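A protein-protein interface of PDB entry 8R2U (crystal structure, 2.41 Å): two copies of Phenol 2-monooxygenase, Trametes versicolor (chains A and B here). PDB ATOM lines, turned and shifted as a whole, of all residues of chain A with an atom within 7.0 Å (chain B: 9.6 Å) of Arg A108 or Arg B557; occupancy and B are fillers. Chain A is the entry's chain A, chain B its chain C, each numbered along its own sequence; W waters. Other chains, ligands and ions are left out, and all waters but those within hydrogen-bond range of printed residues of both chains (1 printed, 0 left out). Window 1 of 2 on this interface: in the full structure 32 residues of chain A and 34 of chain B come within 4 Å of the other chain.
Among the printed residues, pairs that only touch across the chains: Pro A105 with Arg B557, Arg A108 with Arg B557, Pro A110 with Tyr B555 and Pro A110 with Arg B557.
No position is printed for both chains.
The backbone NH of Ala A104 is in hydrogen-bond range of the side-chain hydroxyl of Tyr B555 (3.3 Å). The guanidinium group of Arg B557 sits at hydrogen-bond distance from the backbone carbonyl oxygen of Ala A107, 3.0 Å away.
Of the printed residues of chain B, Ala A104 touches Tyr B555 (3.3 Å). Of the printed residues of chain B, Pro A105 touches Arg B557 (3.6 Å). Asn A106 touches none of the printed residues of chain B. Ala A107 touches just one residue of chain B: Arg B557 (3.0 Å). Arg A108 touches just one residue of chain B: Arg B557 (3.6 Å). Trp A109 touches none of the printed residues of chain B. Of the printed residues of chain B, Pro A110 touches Tyr B555 (3.6 Å) and Arg B557 (3.5 Å). Tyr A462 touches none of the printed residues of chain B. Gln A465 touches none of the printed residues of chain B. Of the printed residues of chain A, Tyr B555 touches Ala A104 (3.3 Å) and Pro A110 (3.6 Å). Arg B557 touches just these residues of chain A: Pro A105, Ala A107, Arg A108 and Pro A110. The nearest residue of chain A that does not touch Arg B557 is Asn A106 (4.6 Å). The nearest printed residue of chain A that does not touch Tyr B555 is Pro A105 (4.3 Å).
The side-chain carboxylate (OE1) of Glu A61 is in hydrogen-bond range of the backbone NH (N) of Arg A108. The side-chain carboxylate (OD2) of Asp A463 lies within salt-bridge range of the guanidinium group (NE) of Arg A108, 3.9 Å away. NH2 of Arg A108 is in salt-bridge range of OD2 of Asp A466 (2.8 Å). N of Tyr B555 sits close to OD2 of Asp B553. N of Arg B557 is in hydrogen-bond range of OD1 of Asp B553 (2.7 Å).
Of the 14 printed residues of chain B, 2 touch a printed residue of chain A. Hydrophobic or aromatic side chains of chain A within 4 Å of the printed part of chain B: Pro A110. Among the printed residues, 6 pairs touch across the chains.
Water W1 bridges the backbone carbonyl oxygen of Arg A108 (3.0 Å) and the guanidinium group of Arg B557 (3.2 Å).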
ATOM      1  N   PRO A  57     -16.634  30.466  -0.818  1.00  0.00           N
ATOM      2  CA  PRO A  57     -15.620  29.580  -0.255  1.00  0.00           C
ATOM      3  C   PRO A  57     -15.668  29.343   1.250  1.00  0.00           C
ATOM      4  O   PRO A  57     -15.599  28.197   1.704  1.00  0.00           O
ATOM      5  CB  PRO A  57     -14.327  30.319  -0.622  1.00  0.00           C
ATOM      6  CG  PRO A  57     -14.635  30.945  -1.975  1.00  0.00           C
ATOM      7  CD  PRO A  57     -16.096  31.338  -1.878  1.00  0.00           C
ATOM      8  N   GLU A  61     -16.575  25.929   3.661  1.00  0.00           N
ATOM      9  CA  GLU A  61     -15.789  25.482   4.803  1.00  0.00           C
ATOM     10  C   GLU A  61     -16.689  25.327   6.021  1.00  0.00           C
ATOM     11  O   GLU A  61     -16.569  24.350   6.755  1.00  0.00           O
ATOM     12  CB  GLU A  61     -14.634  26.438   5.112  1.00  0.00           C
ATOM     13  CG  GLU A  61     -13.578  26.523   3.991  1.00  0.00           C
ATOM     14  CD  GLU A  61     -12.495  27.561   4.193  1.00  0.00           C
ATOM     15  OE1 GLU A  61     -11.649  27.708   3.271  1.00  0.00           O
ATOM     16  OE2 GLU A  61     -12.513  28.242   5.259  1.00  0.00           O
ATOM     17  N   GLN A  64     -18.829  22.401   5.748  1.00  0.00           N
ATOM     18  CA  GLN A  64     -17.959  21.269   5.967  1.00  0.00           C
ATOM     19  C   GLN A  64     -17.862  20.971   7.463  1.00  0.00           C
ATOM     20  O   GLN A  64     -17.875  19.808   7.868  1.00  0.00           O
ATOM     21  CB  GLN A  64     -16.577  21.515   5.371  1.00  0.00           C
ATOM     22  CG  GLN A  64     -15.622  20.348   5.556  1.00  0.00           C
ATOM     23  CD  GLN A  64     -15.896  19.108   4.711  1.00  0.00           C
ATOM     24  OE1 GLN A  64     -16.885  18.964   3.995  1.00  0.00           O
ATOM     25  NE2 GLN A  64     -14.992  18.152   4.772  1.00  0.00           N
ATOM     26  N   SER A  65     -17.794  22.020   8.287  1.00  0.00           N
ATOM     27  CA  SER A  65     -17.681  21.859   9.733  1.00  0.00           C
ATOM     28  C   SER A  65     -18.915  21.172  10.338  1.00  0.00           C
ATOM     29  O   SER A  65     -18.814  20.685  11.462  1.00  0.00           O
ATOM     30  CB  SER A  65     -17.347  23.171  10.459  1.00  0.00           C
ATOM     31  OG  SER A  65     -18.413  24.115  10.448  1.00  0.00           O
ATOM     32  N   ALA A 104      -8.478  33.899  -3.825  1.00  0.00           N
ATOM     33  CA  ALA A 104      -8.247  33.358  -2.495  1.00  0.00           C
ATOM     34  C   ALA A 104      -7.423  32.078  -2.594  1.00  0.00           C
ATOM     35  O   ALA A 104      -7.968  30.969  -2.657  1.00  0.00           O
ATOM     36  CB  ALA A 104      -9.560  33.078  -1.820  1.00  0.00           C
ATOM     37  N   PRO A 105      -6.079  32.193  -2.626  1.00  0.00           N
ATOM     38  CA  PRO A 105      -5.223  31.001  -2.689  1.00  0.00           C
ATOM     39  C   PRO A 105      -5.128  30.175  -1.404  1.00  0.00           C
ATOM     40  O   PRO A 105      -4.568  29.096  -1.453  1.00  0.00           O
ATOM     41  CB  PRO A 105      -3.856  31.597  -3.078  1.00  0.00           C
ATOM     42  CG  PRO A 105      -3.882  33.066  -2.620  1.00  0.00           C
ATOM     43  CD  PRO A 105      -5.341  33.468  -2.644  1.00  0.00           C
ATOM     44  N   ASN A 106      -5.617  30.705  -0.258  1.00  0.00           N
ATOM     45  CA  ASN A 106      -5.793  29.926   0.967  1.00  0.00           C
ATOM     46  C   ASN A 106      -6.866  28.870   0.754  1.00  0.00           C
ATOM     47  O   ASN A 106      -6.734  27.737   1.206  1.00  0.00           O
ATOM     48  CB  ASN A 106      -6.492  30.634   2.134  1.00  0.00           C
ATOM     49  CG  ASN A 106      -6.067  32.059   2.356  1.00  0.00           C
ATOM     50  OD1 ASN A 106      -5.186  32.276   3.188  1.00  0.00           O
ATOM     51  ND2 ASN A 106      -6.756  33.004   1.710  1.00  0.00           N
ATOM     52  N   ALA A 107      -7.940  29.302   0.081  1.00  0.00           N
ATOM     53  CA  ALA A 107      -9.234  28.648   0.118  1.00  0.00           C
ATOM     54  C   ALA A 107      -9.095  27.160  -0.157  1.00  0.00           C
ATOM     55  O   ALA A 107      -8.358  26.717  -1.027  1.00  0.00           O
ATOM     56  CB  ALA A 107     -10.172  29.273  -0.883  1.00  0.00           C
ATOM     57  N   ARG A 108      -9.856  26.394   0.594  1.00  0.00           N
ATOM     58  CA  ARG A 108      -9.901  24.970   0.371  1.00  0.00           C
ATOM     59  C   ARG A 108     -10.652  24.707  -0.936  1.00  0.00           C
ATOM     60  O   ARG A 108     -10.249  23.871  -1.735  1.00  0.00           O
ATOM     61  CB  ARG A 108     -10.570  24.356   1.604  1.00  0.00           C
ATOM     62  CG  ARG A 108      -9.981  23.019   1.960  1.00  0.00           C
ATOM     63  CD  ARG A 108     -10.663  22.501   3.182  1.00  0.00           C
ATOM     64  NE  ARG A 108     -10.622  21.068   3.052  1.00  0.00           N
ATOM     65  CZ  ARG A 108     -11.230  20.231   3.851  1.00  0.00           C
ATOM     66  NH1 ARG A 108     -11.920  20.685   4.887  1.00  0.00           N
ATOM     67  NH2 ARG A 108     -11.132  18.937   3.606  1.00  0.00           N
ATOM     68  N   TRP A 109     -11.766  25.437  -1.120  1.00  0.00           N
ATOM     69  CA  TRP A 109     -12.572  25.414  -2.329  1.00  0.00           C
ATOM     70  C   TRP A 109     -12.580  26.825  -2.914  1.00  0.00           C
ATOM     71  O   TRP A 109     -13.368  27.712  -2.502  1.00  0.00           O
ATOM     72  CB  TRP A 109     -13.985  24.952  -2.012  1.00  0.00           C
ATOM     73  CG  TRP A 109     -14.082  23.543  -1.541  1.00  0.00           C
ATOM     74  CD1 TRP A 109     -14.109  22.424  -2.322  1.00  0.00           C
ATOM     75  CD2 TRP A 109     -14.148  23.097  -0.181  1.00  0.00           C
ATOM     76  NE1 TRP A 109     -14.206  21.309  -1.540  1.00  0.00           N
ATOM     77  CE2 TRP A 109     -14.216  21.688  -0.223  1.00  0.00           C
ATOM     78  CE3 TRP A 109     -14.167  23.745   1.061  1.00  0.00           C
ATOM     79  CZ2 TRP A 109     -14.303  20.915   0.935  1.00  0.00           C
ATOM     80  CZ3 TRP A 109     -14.259  22.987   2.210  1.00  0.00           C
ATOM     81  CH2 TRP A 109     -14.305  21.589   2.136  1.00  0.00           C
ATOM     82  N   PRO A 110     -11.648  27.071  -3.864  1.00  0.00           N
ATOM     83  CA  PRO A 110     -11.477  28.382  -4.474  1.00  0.00           C
ATOM     84  C   PRO A 110     -12.435  28.641  -5.622  1.00  0.00           C
ATOM     85  O   PRO A 110     -12.017  28.917  -6.733  1.00  0.00           O
ATOM     86  CB  PRO A 110     -10.030  28.323  -4.955  1.00  0.00           C
ATOM     87  CG  PRO A 110      -9.839  26.858  -5.351  1.00  0.00           C
ATOM     88  CD  PRO A 110     -10.651  26.101  -4.338  1.00  0.00           C
ATOM     89  N   PHE A 111     -13.724  28.595  -5.309  1.00  0.00           N
ATOM     90  CA  PHE A 111     -14.776  28.912  -6.250  1.00  0.00           C
ATOM     91  C   PHE A 111     -16.054  29.133  -5.469  1.00  0.00           C
ATOM     92  O   PHE A 111     -16.114  28.821  -4.292  1.00  0.00           O
ATOM     93  CB  PHE A 111     -14.979  27.762  -7.230  1.00  0.00           C
ATOM     94  CG  PHE A 111     -15.052  26.362  -6.650  1.00  0.00           C
ATOM     95  CD1 PHE A 111     -16.258  25.827  -6.239  1.00  0.00           C
ATOM     96  CD2 PHE A 111     -13.918  25.563  -6.580  1.00  0.00           C
ATOM     97  CE1 PHE A 111     -16.333  24.533  -5.770  1.00  0.00           C
ATOM     98  CE2 PHE A 111     -13.990  24.261  -6.114  1.00  0.00           C
ATOM     99  CZ  PHE A 111     -15.201  23.745  -5.712  1.00  0.00           C
ATOM    100  N   ILE A 421     -13.271  34.904   3.468  1.00  0.00           N
ATOM    101  CA  ILE A 421     -12.086  34.481   4.183  1.00  0.00           C
ATOM    102  C   ILE A 421     -11.421  35.657   4.900  1.00  0.00           C
ATOM    103  O   ILE A 421     -10.657  35.455   5.836  1.00  0.00           O
ATOM    104  CB  ILE A 421     -11.143  33.787   3.192  1.00  0.00           C
ATOM    105  CG1 ILE A 421     -11.766  32.478   2.728  1.00  0.00           C
ATOM    106  CG2 ILE A 421      -9.751  33.582   3.768  1.00  0.00           C
ATOM    107  CD1 ILE A 421     -11.126  31.911   1.499  1.00  0.00           C
ATOM    108  N   ARG A 447     -10.078  33.027  10.306  1.00  0.00           N
ATOM    109  CA  ARG A 447     -10.387  31.618  10.318  1.00  0.00           C
ATOM    110  C   ARG A 447      -9.086  30.835  10.228  1.00  0.00           C
ATOM    111  O   ARG A 447      -8.099  31.321   9.666  1.00  0.00           O
ATOM    112  CB  ARG A 447     -11.389  31.318   9.204  1.00  0.00           C
ATOM    113  CG  ARG A 447     -10.893  31.490   7.782  1.00  0.00           C
ATOM    114  CD  ARG A 447     -10.093  30.289   7.298  1.00  0.00           C
ATOM    115  NE  ARG A 447     -10.307  29.919   5.908  1.00  0.00           N
ATOM    116  CZ  ARG A 447      -9.371  29.991   4.970  1.00  0.00           C
ATOM    117  NH1 ARG A 447      -8.249  30.659   5.217  1.00  0.00           N
ATOM    118  NH2 ARG A 447      -9.630  29.517   3.761  1.00  0.00           N
ATOM    119  N   PRO A 450      -6.243  26.590   6.276  1.00  0.00           N
ATOM    120  CA  PRO A 450      -6.124  25.233   5.751  1.00  0.00           C
ATOM    121  C   PRO A 450      -4.677  24.863   5.512  1.00  0.00           C
ATOM    122  O   PRO A 450      -3.940  25.676   4.959  1.00  0.00           O
ATOM    123  CB  PRO A 450      -6.826  25.252   4.386  1.00  0.00           C
ATOM    124  CG  PRO A 450      -7.785  26.415   4.484  1.00  0.00           C
ATOM    125  CD  PRO A 450      -7.140  27.411   5.446  1.00  0.00           C
ATOM    126  N   HIS A 451      -4.320  23.652   5.982  1.00  0.00           N
ATOM    127  CA  HIS A 451      -3.111  22.925   5.607  1.00  0.00           C
ATOM    128  C   HIS A 451      -3.331  21.451   5.943  1.00  0.00           C
ATOM    129  O   HIS A 451      -4.108  21.144   6.835  1.00  0.00           O
ATOM    130  CB  HIS A 451      -1.870  23.510   6.277  1.00  0.00           C
ATOM    131  CG  HIS A 451      -0.614  23.125   5.582  1.00  0.00           C
ATOM    132  ND1 HIS A 451      -0.174  23.757   4.447  1.00  0.00           N
ATOM    133  CD2 HIS A 451       0.300  22.163   5.847  1.00  0.00           C
ATOM    134  CE1 HIS A 451       0.939  23.169   4.043  1.00  0.00           C
ATOM    135  NE2 HIS A 451       1.252  22.213   4.885  1.00  0.00           N
ATOM    136  N   TYR A 462      -5.383  14.628   6.546  1.00  0.00           N
ATOM    137  CA  TYR A 462      -6.571  15.411   6.823  1.00  0.00           C
ATOM    138  C   TYR A 462      -6.166  16.868   6.728  1.00  0.00           C
ATOM    139  O   TYR A 462      -5.094  17.247   7.211  1.00  0.00           O
ATOM    140  CB  TYR A 462      -7.088  15.191   8.242  1.00  0.00           C
ATOM    141  CG  TYR A 462      -7.938  13.963   8.463  1.00  0.00           C
ATOM    142  CD1 TYR A 462      -9.299  13.998   8.234  1.00  0.00           C
ATOM    143  CD2 TYR A 462      -7.385  12.779   8.913  1.00  0.00           C
ATOM    144  CE1 TYR A 462     -10.098  12.896   8.480  1.00  0.00           C
ATOM    145  CE2 TYR A 462      -8.160  11.658   9.151  1.00  0.00           C
ATOM    146  CZ  TYR A 462      -9.520  11.722   8.934  1.00  0.00           C
ATOM    147  OH  TYR A 462     -10.288  10.633   9.136  1.00  0.00           O
ATOM    148  N   ASP A 463      -7.033  17.690   6.129  1.00  0.00           N
ATOM    149  CA  ASP A 463      -6.862  19.112   6.285  1.00  0.00           C
ATOM    150  C   ASP A 463      -7.168  19.425   7.739  1.00  0.00           C
ATOM    151  O   ASP A 463      -8.036  18.816   8.343  1.00  0.00           O
ATOM    152  CB  ASP A 463      -7.735  19.855   5.281  1.00  0.00           C
ATOM    153  CG  ASP A 463      -7.326  21.303   5.121  1.00  0.00           C
ATOM    154  OD1 ASP A 463      -7.468  22.049   6.135  1.00  0.00           O
ATOM    155  OD2 ASP A 463      -6.836  21.660   4.009  1.00  0.00           O
ATOM    156  N   ILE A 464      -6.437  20.367   8.304  1.00  0.00           N
ATOM    157  CA  ILE A 464      -6.643  20.727   9.697  1.00  0.00           C
ATOM    158  C   ILE A 464      -8.091  21.148   9.889  1.00  0.00           C
ATOM    159  O   ILE A 464      -8.639  21.023  10.977  1.00  0.00           O
ATOM    160  CB  ILE A 464      -5.669  21.833  10.149  1.00  0.00           C
ATOM    161  CG1 ILE A 464      -5.555  21.904  11.666  1.00  0.00           C
ATOM    162  CG2 ILE A 464      -6.041  23.162   9.528  1.00  0.00           C
ATOM    163  CD1 ILE A 464      -4.859  20.724  12.276  1.00  0.00           C
ATOM    164  N   GLN A 465      -8.729  21.673   8.851  1.00  0.00           N
ATOM    165  CA  GLN A 465     -10.094  22.148   9.027  1.00  0.00           C
ATOM    166  C   GLN A 465     -11.013  20.969   9.323  1.00  0.00           C
ATOM    167  O   GLN A 465     -11.998  21.119  10.064  1.00  0.00           O
ATOM    168  CB  GLN A 465     -10.598  22.929   7.808  1.00  0.00           C
ATOM    169  CG  GLN A 465     -10.098  24.373   7.749  1.00  0.00           C
ATOM    170  CD  GLN A 465     -10.768  25.211   6.685  1.00  0.00           C
ATOM    171  OE1 GLN A 465     -11.399  24.721   5.748  1.00  0.00           O
ATOM    172  NE2 GLN A 465     -10.606  26.511   6.825  1.00  0.00           N
ATOM    173  N   ASP A 466     -10.665  19.793   8.780  1.00  0.00           N
ATOM    174  CA  ASP A 466     -11.492  18.628   8.995  1.00  0.00           C
ATOM    175  C   ASP A 466     -11.362  18.137  10.422  1.00  0.00           C
ATOM    176  O   ASP A 466     -12.158  17.286  10.782  1.00  0.00           O
ATOM    177  CB  ASP A 466     -11.140  17.472   8.069  1.00  0.00           C
ATOM    178  CG  ASP A 466     -11.717  17.653   6.683  1.00  0.00           C
ATOM    179  OD1 ASP A 466     -12.718  18.354   6.590  1.00  0.00           O
ATOM    180  OD2 ASP A 466     -11.147  17.121   5.730  1.00  0.00           O
ATOM    181  N   VAL A 467     -10.375  18.601  11.207  1.00  0.00           N
ATOM    182  CA  VAL A 467     -10.298  18.200  12.605  1.00  0.00           C
ATOM    183  C   VAL A 467     -10.820  19.317  13.499  1.00  0.00           C
ATOM    184  O   VAL A 467     -10.719  19.222  14.725  1.00  0.00           O
ATOM    185  CB  VAL A 467      -8.903  17.698  13.039  1.00  0.00           C
ATOM    186  CG1 VAL A 467      -8.455  16.509  12.215  1.00  0.00           C
ATOM    187  CG2 VAL A 467      -7.836  18.759  13.022  1.00  0.00           C
ATOM    188  N   VAL B 452      -6.618  13.970 -14.717  1.00  0.00           N
ATOM    189  CA  VAL B 452      -7.562  15.072 -14.634  1.00  0.00           C
ATOM    190  C   VAL B 452      -7.523  15.901 -15.919  1.00  0.00           C
ATOM    191  O   VAL B 452      -6.456  16.272 -16.420  1.00  0.00           O
ATOM    192  CB  VAL B 452      -7.266  15.966 -13.424  1.00  0.00           C
ATOM    193  CG1 VAL B 452      -8.221  17.145 -13.362  1.00  0.00           C
ATOM    194  CG2 VAL B 452      -7.293  15.180 -12.128  1.00  0.00           C
ATOM    195  N   VAL B 454     -10.112  19.289 -17.791  1.00  0.00           N
ATOM    196  CA  VAL B 454     -10.872  20.456 -17.404  1.00  0.00           C
ATOM    197  C   VAL B 454     -11.895  20.736 -18.494  1.00  0.00           C
ATOM    198  O   VAL B 454     -11.572  20.700 -19.670  1.00  0.00           O
ATOM    199  CB  VAL B 454      -9.893  21.628 -17.245  1.00  0.00           C
ATOM    200  CG1 VAL B 454     -10.583  22.958 -17.145  1.00  0.00           C
ATOM    201  CG2 VAL B 454      -9.009  21.422 -16.037  1.00  0.00           C
ATOM    202  N   PRO B 461     -12.511  21.030 -13.135  1.00  0.00           N
ATOM    203  CA  PRO B 461     -11.736  19.818 -13.364  1.00  0.00           C
ATOM    204  C   PRO B 461     -12.479  18.544 -13.001  1.00  0.00           C
ATOM    205  O   PRO B 461     -13.271  18.536 -12.093  1.00  0.00           O
ATOM    206  CB  PRO B 461     -10.547  20.036 -12.428  1.00  0.00           C
ATOM    207  CG  PRO B 461     -11.149  20.703 -11.250  1.00  0.00           C
ATOM    208  CD  PRO B 461     -12.185  21.635 -11.837  1.00  0.00           C
ATOM    209  N   LYS B 528      -7.851  26.746 -22.086  1.00  0.00           N
ATOM    210  CA  LYS B 528      -9.148  27.410 -22.066  1.00  0.00           C
ATOM    211  C   LYS B 528      -9.051  28.852 -22.564  1.00  0.00           C
ATOM    212  O   LYS B 528     -10.011  29.384 -23.125  1.00  0.00           O
ATOM    213  CB  LYS B 528      -9.694  27.395 -20.646  1.00  0.00           C
ATOM    214  CG  LYS B 528      -8.826  28.116 -19.627  1.00  0.00           C
ATOM    215  CD  LYS B 528      -9.267  27.845 -18.188  1.00  0.00           C
ATOM    216  CE  LYS B 528      -8.067  27.713 -17.281  1.00  0.00           C
ATOM    217  NZ  LYS B 528      -7.602  26.317 -17.333  1.00  0.00           N
ATOM    218  N   ASP B 551      -5.602  20.747 -19.777  1.00  0.00           N
ATOM    219  CA  ASP B 551      -5.278  22.032 -19.197  1.00  0.00           C
ATOM    220  C   ASP B 551      -5.470  21.915 -17.693  1.00  0.00           C
ATOM    221  O   ASP B 551      -6.110  20.963 -17.250  1.00  0.00           O
ATOM    222  CB  ASP B 551      -6.168  23.134 -19.787  1.00  0.00           C
ATOM    223  CG  ASP B 551      -5.716  24.561 -19.513  1.00  0.00           C
ATOM    224  OD1 ASP B 551      -4.526  24.755 -19.173  1.00  0.00           O
ATOM    225  OD2 ASP B 551      -6.565  25.483 -19.664  1.00  0.00           O
ATOM    226  N   THR B 552      -4.931  22.879 -16.921  1.00  0.00           N
ATOM    227  CA  THR B 552      -5.062  22.860 -15.466  1.00  0.00           C
ATOM    228  C   THR B 552      -6.339  23.562 -15.021  1.00  0.00           C
ATOM    229  O   THR B 552      -6.925  24.319 -15.780  1.00  0.00           O
ATOM    230  CB  THR B 552      -3.885  23.536 -14.773  1.00  0.00           C
ATOM    231  OG1 THR B 552      -3.838  24.895 -15.181  1.00  0.00           O
ATOM    232  CG2 THR B 552      -2.565  22.890 -15.113  1.00  0.00           C
ATOM    233  N   ASP B 553      -6.782  23.291 -13.795  1.00  0.00           N
ATOM    234  CA  ASP B 553      -7.790  24.115 -13.170  1.00  0.00           C
ATOM    235  C   ASP B 553      -7.193  25.515 -13.023  1.00  0.00           C
ATOM    236  O   ASP B 553      -6.003  25.706 -13.262  1.00  0.00           O
ATOM    237  CB  ASP B 553      -8.230  23.529 -11.829  1.00  0.00           C
ATOM    238  CG  ASP B 553      -7.206  23.782 -10.737  1.00  0.00           C
ATOM    239  OD1 ASP B 553      -5.996  23.494 -10.996  1.00  0.00           O
ATOM    240  OD2 ASP B 553      -7.601  24.365  -9.683  1.00  0.00           O
ATOM    241  N   LEU B 554      -8.013  26.463 -12.568  1.00  0.00           N
ATOM    242  CA  LEU B 554      -7.667  27.872 -12.603  1.00  0.00           C
ATOM    243  C   LEU B 554      -6.529  28.228 -11.654  1.00  0.00           C
ATOM    244  O   LEU B 554      -5.892  29.247 -11.878  1.00  0.00           O
ATOM    245  CB  LEU B 554      -8.916  28.687 -12.264  1.00  0.00           C
ATOM    246  CG  LEU B 554      -9.937  28.752 -13.395  1.00  0.00           C
ATOM    247  CD1 LEU B 554     -11.305  29.151 -12.878  1.00  0.00           C
ATOM    248  CD2 LEU B 554      -9.486  29.703 -14.476  1.00  0.00           C
ATOM    249  N   TYR B 555      -6.299  27.434 -10.601  1.00  0.00           N
ATOM    250  CA  TYR B 555      -5.243  27.700  -9.620  1.00  0.00           C
ATOM    251  C   TYR B 555      -4.008  26.830  -9.854  1.00  0.00           C
ATOM    252  O   TYR B 555      -3.121  26.759  -8.985  1.00  0.00           O
ATOM    253  CB  TYR B 555      -5.780  27.548  -8.194  1.00  0.00           C
ATOM    254  CG  TYR B 555      -6.537  28.771  -7.749  1.00  0.00           C
ATOM    255  CD1 TYR B 555      -7.834  28.965  -8.179  1.00  0.00           C
ATOM    256  CD2 TYR B 555      -5.914  29.802  -7.065  1.00  0.00           C
ATOM    257  CE1 TYR B 555      -8.557  30.081  -7.789  1.00  0.00           C
ATOM    258  CE2 TYR B 555      -6.601  30.953  -6.725  1.00  0.00           C
ATOM    259  CZ  TYR B 555      -7.935  31.088  -7.070  1.00  0.00           C
ATOM    260  OH  TYR B 555      -8.616  32.224  -6.679  1.00  0.00           O
ATOM    261  N   ALA B 556      -3.974  26.180 -11.037  1.00  0.00           N
ATOM    262  CA  ALA B 556      -2.904  25.277 -11.451  1.00  0.00           C
ATOM    263  C   ALA B 556      -2.603  24.262 -10.338  1.00  0.00           C
ATOM    264  O   ALA B 556      -1.450  24.034  -9.984  1.00  0.00           O
ATOM    265  CB  ALA B 556      -1.670  26.059 -11.852  1.00  0.00           C
ATOM    266  N   ARG B 557      -3.650  23.669  -9.766  1.00  0.00           N
ATOM    267  CA  ARG B 557      -3.468  22.665  -8.723  1.00  0.00           C
ATOM    268  C   ARG B 557      -3.546  21.256  -9.312  1.00  0.00           C
ATOM    269  O   ARG B 557      -2.930  20.336  -8.786  1.00  0.00           O
ATOM    270  CB  ARG B 557      -4.535  22.795  -7.623  1.00  0.00           C
ATOM    271  CG  ARG B 557      -4.396  24.022  -6.728  1.00  0.00           C
ATOM    272  CD  ARG B 557      -5.607  24.163  -5.839  1.00  0.00           C
ATOM    273  NE  ARG B 557      -5.589  25.329  -4.991  1.00  0.00           N
ATOM    274  CZ  ARG B 557      -6.498  25.544  -4.044  1.00  0.00           C
ATOM    275  NH1 ARG B 557      -7.498  24.689  -3.868  1.00  0.00           N
ATOM    276  NH2 ARG B 557      -6.395  26.597  -3.251  1.00  0.00           N
ATOM    277  N   VAL B 558      -4.373  21.086 -10.349  1.00  0.00           N
ATOM    278  CA  VAL B 558      -4.587  19.790 -10.953  1.00  0.00           C
ATOM    279  C   VAL B 558      -4.693  19.975 -12.458  1.00  0.00           C
ATOM    280  O   VAL B 558      -4.869  21.093 -12.928  1.00  0.00           O
ATOM    281  CB  VAL B 558      -5.856  19.130 -10.406  1.00  0.00           C
ATOM    282  CG1 VAL B 558      -5.795  18.938  -8.904  1.00  0.00           C
ATOM    283  CG2 VAL B 558      -7.094  19.892 -10.800  1.00  0.00           C
ATOM    284  N   GLY B 559      -4.598  18.862 -13.192  1.00  0.00           N
ATOM    285  CA  GLY B 559      -4.775  18.873 -14.631  1.00  0.00           C
ATOM    286  C   GLY B 559      -3.491  19.212 -15.354  1.00  0.00           C
ATOM    287  O   GLY B 559      -2.474  19.455 -14.705  1.00  0.00           O
ATOM    288  N   GLY B 560      -3.590  19.231 -16.696  1.00  0.00           N
ATOM    289  CA  GLY B 560      -2.434  19.352 -17.568  1.00  0.00           C
ATOM    290  C   GLY B 560      -1.755  18.011 -17.751  1.00  0.00           C
ATOM    291  O   GLY B 560      -1.980  17.104 -16.951  1.00  0.00           O
HETATM  292  O   HOH W   1      -7.601  22.585  -1.394  1.00  0.00           O
